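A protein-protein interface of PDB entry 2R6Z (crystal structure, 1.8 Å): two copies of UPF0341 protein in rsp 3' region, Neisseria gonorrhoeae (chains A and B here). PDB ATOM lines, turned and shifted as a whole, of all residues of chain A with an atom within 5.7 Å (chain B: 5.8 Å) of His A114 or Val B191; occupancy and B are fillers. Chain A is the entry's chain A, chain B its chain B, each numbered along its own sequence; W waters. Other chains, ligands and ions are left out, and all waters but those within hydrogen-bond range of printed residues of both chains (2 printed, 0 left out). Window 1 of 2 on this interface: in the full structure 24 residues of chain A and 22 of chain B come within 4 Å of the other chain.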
ATOM      1  N   THR A   2      18.960   0.620  29.558  1.00  0.00           N
ATOM      2  CA  THR A   2      18.314   0.372  28.241  1.00  0.00           C
ATOM      3  C   THR A   2      17.047   1.207  28.127  1.00  0.00           C
ATOM      4  O   THR A   2      16.170   1.150  28.998  1.00  0.00           O
ATOM      5  CB  THR A   2      17.939  -1.121  28.072  1.00  0.00           C
ATOM      6  OG1 THR A   2      19.118  -1.933  28.151  1.00  0.00           O
ATOM      7  CG2 THR A   2      17.271  -1.356  26.727  1.00  0.00           C
ATOM      8  N   SER A  34      21.439   2.133  20.470  1.00  0.00           N
ATOM      9  CA  SER A  34      20.266   1.275  20.416  1.00  0.00           C
ATOM     10  C   SER A  34      19.191   1.619  21.438  1.00  0.00           C
ATOM     11  O   SER A  34      19.398   2.426  22.347  1.00  0.00           O
ATOM     12  CB  SER A  34      20.689  -0.182  20.637  1.00  0.00           C
ATOM     13  OG  SER A  34      21.316  -0.345  21.915  1.00  0.00           O
ATOM     14  N   LEU A  45      14.451  -4.561  18.905  1.00  0.00           N
ATOM     15  CA  LEU A  45      15.624  -3.758  19.211  1.00  0.00           C
ATOM     16  C   LEU A  45      16.014  -2.951  17.977  1.00  0.00           C
ATOM     17  O   LEU A  45      16.040  -3.467  16.855  1.00  0.00           O
ATOM     18  CB  LEU A  45      16.787  -4.647  19.655  1.00  0.00           C
ATOM     19  CG  LEU A  45      18.068  -3.967  20.170  1.00  0.00           C
ATOM     20  CD1 LEU A  45      17.746  -3.071  21.367  1.00  0.00           C
ATOM     21  CD2 LEU A  45      19.064  -5.038  20.571  1.00  0.00           C
ATOM     22  N   GLU A 112      18.783 -14.966  31.642  1.00  0.00           N
ATOM     23  CA  GLU A 112      19.413 -13.889  30.862  1.00  0.00           C
ATOM     24  C   GLU A 112      19.510 -12.678  31.780  1.00  0.00           C
ATOM     25  O   GLU A 112      18.510 -12.257  32.357  1.00  0.00           O
ATOM     26  CB  GLU A 112      18.585 -13.536  29.627  1.00  0.00           C
ATOM     27  CG  GLU A 112      19.133 -12.355  28.825  1.00  0.00           C
ATOM     28  CD  GLU A 112      20.590 -12.533  28.444  1.00  0.00           C
ATOM     29  OE1 GLU A 112      20.934 -13.608  27.916  1.00  0.00           O
ATOM     30  OE2 GLU A 112      21.389 -11.597  28.656  1.00  0.00           O
ATOM     31  N   GLN A 113      20.711 -12.119  31.907  1.00  0.00           N
ATOM     32  CA  GLN A 113      20.934 -10.981  32.792  1.00  0.00           C
ATOM     33  C   GLN A 113      20.816  -9.605  32.143  1.00  0.00           C
ATOM     34  O   GLN A 113      20.625  -8.608  32.841  1.00  0.00           O
ATOM     35  CB  GLN A 113      22.311 -11.096  33.446  1.00  0.00           C
ATOM     36  CG  GLN A 113      23.459 -10.910  32.481  1.00  0.00           C
ATOM     37  CD  GLN A 113      24.802 -11.247  33.101  1.00  0.00           C
ATOM     38  OE1 GLN A 113      25.211 -10.641  34.091  1.00  0.00           O
ATOM     39  NE2 GLN A 113      25.490 -12.224  32.524  1.00  0.00           N
ATOM     40  N   HIS A 114      20.952  -9.530  30.825  1.00  0.00           N
ATOM     41  CA  HIS A 114      20.849  -8.232  30.166  1.00  0.00           C
ATOM     42  C   HIS A 114      19.381  -7.842  29.999  1.00  0.00           C
ATOM     43  O   HIS A 114      18.590  -8.597  29.439  1.00  0.00           O
ATOM     44  CB  HIS A 114      21.540  -8.256  28.805  1.00  0.00           C
ATOM     45  CG  HIS A 114      21.730  -6.896  28.217  1.00  0.00           C
ATOM     46  ND1 HIS A 114      22.978  -6.306  28.092  1.00  0.00           N
ATOM     47  CD2 HIS A 114      20.843  -5.985  27.770  1.00  0.00           C
ATOM     48  CE1 HIS A 114      22.837  -5.095  27.596  1.00  0.00           C
ATOM     49  NE2 HIS A 114      21.550  -4.869  27.389  1.00  0.00           N
ATOM     50  N   PRO A 115      18.999  -6.647  30.479  1.00  0.00           N
ATOM     51  CA  PRO A 115      17.615  -6.159  30.390  1.00  0.00           C
ATOM     52  C   PRO A 115      17.000  -6.178  28.998  1.00  0.00           C
ATOM     53  O   PRO A 115      15.867  -6.624  28.816  1.00  0.00           O
ATOM     54  CB  PRO A 115      17.712  -4.740  30.939  1.00  0.00           C
ATOM     55  CG  PRO A 115      18.833  -4.832  31.916  1.00  0.00           C
ATOM     56  CD  PRO A 115      19.855  -5.651  31.144  1.00  0.00           C
ATOM     57  N   ALA A 116      17.746  -5.679  28.019  1.00  0.00           N
ATOM     58  CA  ALA A 116      17.262  -5.625  26.648  1.00  0.00           C
ATOM     59  C   ALA A 116      17.089  -7.014  26.047  1.00  0.00           C
ATOM     60  O   ALA A 116      16.036  -7.335  25.492  1.00  0.00           O
ATOM     61  CB  ALA A 116      18.220  -4.805  25.789  1.00  0.00           C
ATOM     62  N   VAL A 117      18.128  -7.835  26.155  1.00  0.00           N
ATOM     63  CA  VAL A 117      18.086  -9.191  25.614  1.00  0.00           C
ATOM     64  C   VAL A 117      16.965  -9.990  26.277  1.00  0.00           C
ATOM     65  O   VAL A 117      16.189 -10.681  25.607  1.00  0.00           O
ATOM     66  CB  VAL A 117      19.440  -9.909  25.831  1.00  0.00           C
ATOM     67  CG1 VAL A 117      19.399 -11.311  25.223  1.00  0.00           C
ATOM     68  CG2 VAL A 117      20.563  -9.090  25.188  1.00  0.00           C
ATOM     69  N   ALA A 118      16.888  -9.899  27.600  1.00  0.00           N
ATOM     70  CA  ALA A 118      15.855 -10.603  28.346  1.00  0.00           C
ATOM     71  C   ALA A 118      14.461 -10.151  27.912  1.00  0.00           C
ATOM     72  O   ALA A 118      13.544 -10.969  27.756  1.00  0.00           O
ATOM     73  CB  ALA A 118      16.030 -10.361  29.847  1.00  0.00           C
ATOM     74  N   CYS A 119      14.287  -8.846  27.730  1.00  0.00           N
ATOM     75  CA  CYS A 119      12.979  -8.339  27.329  1.00  0.00           C
ATOM     76  C   CYS A 119      12.605  -8.891  25.951  1.00  0.00           C
ATOM     77  O   CYS A 119      11.471  -9.335  25.731  1.00  0.00           O
ATOM     78  CB  CYS A 119      12.988  -6.807  27.309  1.00  0.00           C
ATOM     79  SG  CYS A 119      11.324  -6.110  27.100  1.00  0.00           S
ATOM     80  N   PHE A 145      14.911 -13.684  34.639  1.00  0.00           N
ATOM     81  CA  PHE A 145      15.768 -12.516  34.460  1.00  0.00           C
ATOM     82  C   PHE A 145      16.799 -12.397  35.574  1.00  0.00           C
ATOM     83  O   PHE A 145      16.461 -12.477  36.757  1.00  0.00           O
ATOM     84  CB  PHE A 145      14.924 -11.237  34.411  1.00  0.00           C
ATOM     85  CG  PHE A 145      15.737  -9.971  34.323  1.00  0.00           C
ATOM     86  CD1 PHE A 145      16.635  -9.773  33.277  1.00  0.00           C
ATOM     87  CD2 PHE A 145      15.604  -8.977  35.291  1.00  0.00           C
ATOM     88  CE1 PHE A 145      17.389  -8.604  33.194  1.00  0.00           C
ATOM     89  CE2 PHE A 145      16.355  -7.801  35.219  1.00  0.00           C
ATOM     90  CZ  PHE A 145      17.247  -7.617  34.170  1.00  0.00           C
ATOM     91  N   TYR B 186      26.518  -7.824  14.559  1.00  0.00           N
ATOM     92  CA  TYR B 186      25.648  -6.654  14.578  1.00  0.00           C
ATOM     93  C   TYR B 186      24.895  -6.548  15.900  1.00  0.00           C
ATOM     94  O   TYR B 186      24.790  -5.472  16.490  1.00  0.00           O
ATOM     95  CB  TYR B 186      24.642  -6.734  13.427  1.00  0.00           C
ATOM     96  CG  TYR B 186      23.747  -5.523  13.317  1.00  0.00           C
ATOM     97  CD1 TYR B 186      24.258  -4.289  12.921  1.00  0.00           C
ATOM     98  CD2 TYR B 186      22.388  -5.610  13.611  1.00  0.00           C
ATOM     99  CE1 TYR B 186      23.438  -3.167  12.817  1.00  0.00           C
ATOM    100  CE2 TYR B 186      21.559  -4.495  13.512  1.00  0.00           C
ATOM    101  CZ  TYR B 186      22.089  -3.279  13.115  1.00  0.00           C
ATOM    102  OH  TYR B 186      21.275  -2.175  13.009  1.00  0.00           O
ATOM    103  N   PHE B 187      24.367  -7.677  16.359  1.00  0.00           N
ATOM    104  CA  PHE B 187      23.619  -7.708  17.606  1.00  0.00           C
ATOM    105  C   PHE B 187      24.495  -7.337  18.804  1.00  0.00           C
ATOM    106  O   PHE B 187      24.044  -6.655  19.726  1.00  0.00           O
ATOM    107  CB  PHE B 187      23.000  -9.098  17.801  1.00  0.00           C
ATOM    108  CG  PHE B 187      22.228  -9.243  19.079  1.00  0.00           C
ATOM    109  CD1 PHE B 187      22.773  -9.926  20.161  1.00  0.00           C
ATOM    110  CD2 PHE B 187      20.960  -8.687  19.207  1.00  0.00           C
ATOM    111  CE1 PHE B 187      22.072 -10.049  21.353  1.00  0.00           C
ATOM    112  CE2 PHE B 187      20.250  -8.804  20.396  1.00  0.00           C
ATOM    113  CZ  PHE B 187      20.807  -9.489  21.471  1.00  0.00           C
ATOM    114  N   HIS B 188      25.750  -7.777  18.788  1.00  0.00           N
ATOM    115  CA  HIS B 188      26.653  -7.470  19.890  1.00  0.00           C
ATOM    116  C   HIS B 188      26.972  -5.978  19.967  1.00  0.00           C
ATOM    117  O   HIS B 188      27.204  -5.445  21.050  1.00  0.00           O
ATOM    118  CB  HIS B 188      27.939  -8.300  19.772  1.00  0.00           C
ATOM    119  CG  HIS B 188      27.745  -9.757  20.084  1.00  0.00           C
ATOM    120  ND1 HIS B 188      28.793 -10.644  20.189  1.00  0.00           N
ATOM    121  CD2 HIS B 188      26.618 -10.475  20.315  1.00  0.00           C
ATOM    122  CE1 HIS B 188      28.323 -11.849  20.472  1.00  0.00           C
ATOM    123  NE2 HIS B 188      27.007 -11.772  20.553  1.00  0.00           N
ATOM    124  N   ARG B 189      26.974  -5.307  18.820  1.00  0.00           N
ATOM    125  CA  ARG B 189      27.239  -3.870  18.771  1.00  0.00           C
ATOM    126  C   ARG B 189      26.073  -3.107  19.396  1.00  0.00           C
ATOM    127  O   ARG B 189      26.244  -1.999  19.915  1.00  0.00           O
ATOM    128  CB  ARG B 189      27.405  -3.403  17.324  1.00  0.00           C
ATOM    129  CG  ARG B 189      27.442  -1.893  17.182  1.00  0.00           C
ATOM    130  CD  ARG B 189      27.260  -1.443  15.749  1.00  0.00           C
ATOM    131  NE  ARG B 189      27.061   0.001  15.681  1.00  0.00           N
ATOM    132  CZ  ARG B 189      26.852   0.678  14.556  1.00  0.00           C
ATOM    133  NH1 ARG B 189      26.814   0.043  13.393  1.00  0.00           N
ATOM    134  NH2 ARG B 189      26.678   1.991  14.593  1.00  0.00           N
ATOM    135  N   LEU B 190      24.888  -3.706  19.340  1.00  0.00           N
ATOM    136  CA  LEU B 190      23.692  -3.079  19.884  1.00  0.00           C
ATOM    137  C   LEU B 190      23.534  -3.227  21.391  1.00  0.00           C
ATOM    138  O   LEU B 190      22.967  -2.354  22.040  1.00  0.00           O
ATOM    139  CB  LEU B 190      22.446  -3.639  19.195  1.00  0.00           C
ATOM    140  CG  LEU B 190      22.412  -3.525  17.666  1.00  0.00           C
ATOM    141  CD1 LEU B 190      21.106  -4.100  17.132  1.00  0.00           C
ATOM    142  CD2 LEU B 190      22.565  -2.083  17.265  1.00  0.00           C
ATOM    143  N   VAL B 191      24.029  -4.318  21.956  1.00  0.00           N
ATOM    144  CA  VAL B 191      23.881  -4.517  23.394  1.00  0.00           C
ATOM    145  C   VAL B 191      25.191  -4.657  24.155  1.00  0.00           C
ATOM    146  O   VAL B 191      25.194  -4.670  25.382  1.00  0.00           O
ATOM    147  CB  VAL B 191      23.030  -5.763  23.699  1.00  0.00           C
ATOM    148  CG1 VAL B 191      21.621  -5.573  23.182  1.00  0.00           C
ATOM    149  CG2 VAL B 191      23.674  -6.991  23.071  1.00  0.00           C
ATOM    150  N   GLY B 192      26.300  -4.759  23.430  1.00  0.00           N
ATOM    151  CA  GLY B 192      27.587  -4.930  24.079  1.00  0.00           C
ATOM    152  C   GLY B 192      28.351  -3.674  24.438  1.00  0.00           C
ATOM    153  O   GLY B 192      27.777  -2.603  24.658  1.00  0.00           O
ATOM    154  N   GLU B 193      29.671  -3.814  24.495  1.00  0.00           N
ATOM    155  CA  GLU B 193      30.536  -2.694  24.832  1.00  0.00           C
ATOM    156  C   GLU B 193      30.357  -1.484  23.920  1.00  0.00           C
ATOM    157  O   GLU B 193      30.534  -0.359  24.359  1.00  0.00           O
ATOM    158  CB  GLU B 193      32.002  -3.152  24.827  1.00  0.00           C
ATOM    159  CG  GLU B 193      32.413  -3.908  23.576  1.00  0.00           C
ATOM    160  CD  GLU B 193      33.800  -4.519  23.687  1.00  0.00           C
ATOM    161  OE1 GLU B 193      34.211  -5.232  22.742  1.00  0.00           O
ATOM    162  OE2 GLU B 193      34.479  -4.288  24.717  1.00  0.00           O
ATOM    163  N   GLN B 195      27.609  -0.274  22.623  1.00  0.00           N
ATOM    164  CA  GLN B 195      26.475   0.490  23.120  1.00  0.00           C
ATOM    165  C   GLN B 195      26.869   1.135  24.441  1.00  0.00           C
ATOM    166  O   GLN B 195      26.543   2.294  24.692  1.00  0.00           O
ATOM    167  CB  GLN B 195      25.268  -0.440  23.292  1.00  0.00           C
ATOM    168  CG  GLN B 195      24.037   0.177  23.961  1.00  0.00           C
ATOM    169  CD  GLN B 195      23.511   1.409  23.246  1.00  0.00           C
ATOM    170  OE1 GLN B 195      23.771   1.618  22.060  1.00  0.00           O
ATOM    171  NE2 GLN B 195      22.750   2.225  23.969  1.00  0.00           N
ATOM    172  N   ASP B 196      27.577   0.402  25.295  1.00  0.00           N
ATOM    173  CA  ASP B 196      27.990   0.998  26.564  1.00  0.00           C
ATOM    174  C   ASP B 196      28.865   2.228  26.319  1.00  0.00           C
ATOM    175  O   ASP B 196      28.799   3.209  27.069  1.00  0.00           O
ATOM    176  CB  ASP B 196      28.747  -0.010  27.429  1.00  0.00           C
ATOM    177  CG  ASP B 196      27.901  -1.217  27.778  1.00  0.00           C
ATOM    178  OD1 ASP B 196      26.688  -1.039  28.018  1.00  0.00           O
ATOM    179  OD2 ASP B 196      28.451  -2.329  27.821  1.00  0.00           O
HETATM  180  O   HOH W   1      23.717  -2.373  26.575  1.00  0.00           O
HETATM  181  O   HOH W   2      21.225   4.430  22.899  1.00  0.00           O
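The backbone carbonyl oxygen of Leu B190 lies within hydrogen-bond range of the side-chain hydroxyl of Ser A34. OE1 of Gln B195 is in hydrogen-bond range of N of Ser A34 (2.9 Å).
OE2 of Glu A112 is in hydrogen-bond range of N of His A114 (3.0 Å). The backbone carbonyl oxygen of Arg B189 lies within hydrogen-bond range of the backbone NH of Gln B195.
Among the printed residues, pairs that only touch across the chains: His A114 with Val B191 (3.3 Å), Leu A45 with Val B191 (3.7 Å), Val A117 with Phe B187 (3.7 Å), Leu A45 with Leu B190 (3.9 Å) and Leu A45 with Phe B187 (3.95 Å).
Of chain B, only Val B191 (3.3 Å) comes within 4 Å of His A114. Val B191 touches two residues of chain A. Of the printed residues of chain B, Leu A45 touches Phe B187 (3.95 Å), Leu B190 (3.9 Å) and Val B191 (3.7 Å). Of the printed residues of chain A, Leu B190 touches Ser A34 and Leu A45. Of the printed residues of chain B, Val A117 touches Phe B187 (3.7 Å). Of the printed residues of chain A, Phe B187 touches Leu A45 and Val A117. Of the printed residues of chain B, Ser A34 touches Leu B190 and Gln B195. Phe A145 touches none of the printed residues of chain B.
Hydrophobic or aromatic side chains of chain B that line the printed part of chain A: Phe B187, Leu B190 and Val B191. Printed residues of chain A that touch a printed residue of chain B: Ser A34, Leu A45, His A114 and Val A117. Among the printed residues, 7 pairs touch across the chains. Among the printed residues, no Asp or Glu carboxylate lies within 4 Å of a Lys or Arg side-chain nitrogen of the other chain.
No position is printed for both chains. Of the 7 pairs that touch across the chains among the printed residues, none has its exchanged pair printed and touching as well.
Water W2 lies within hydrogen-bond range of the backbone carbonyl oxygen of Ser A34 (2.8 Å) and the side-chain amide nitrogen of Gln B195 (2.9 Å). Water W1 bridges O of Val B191 (3.0 Å) and NE2 of His A114 (3.4 Å).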
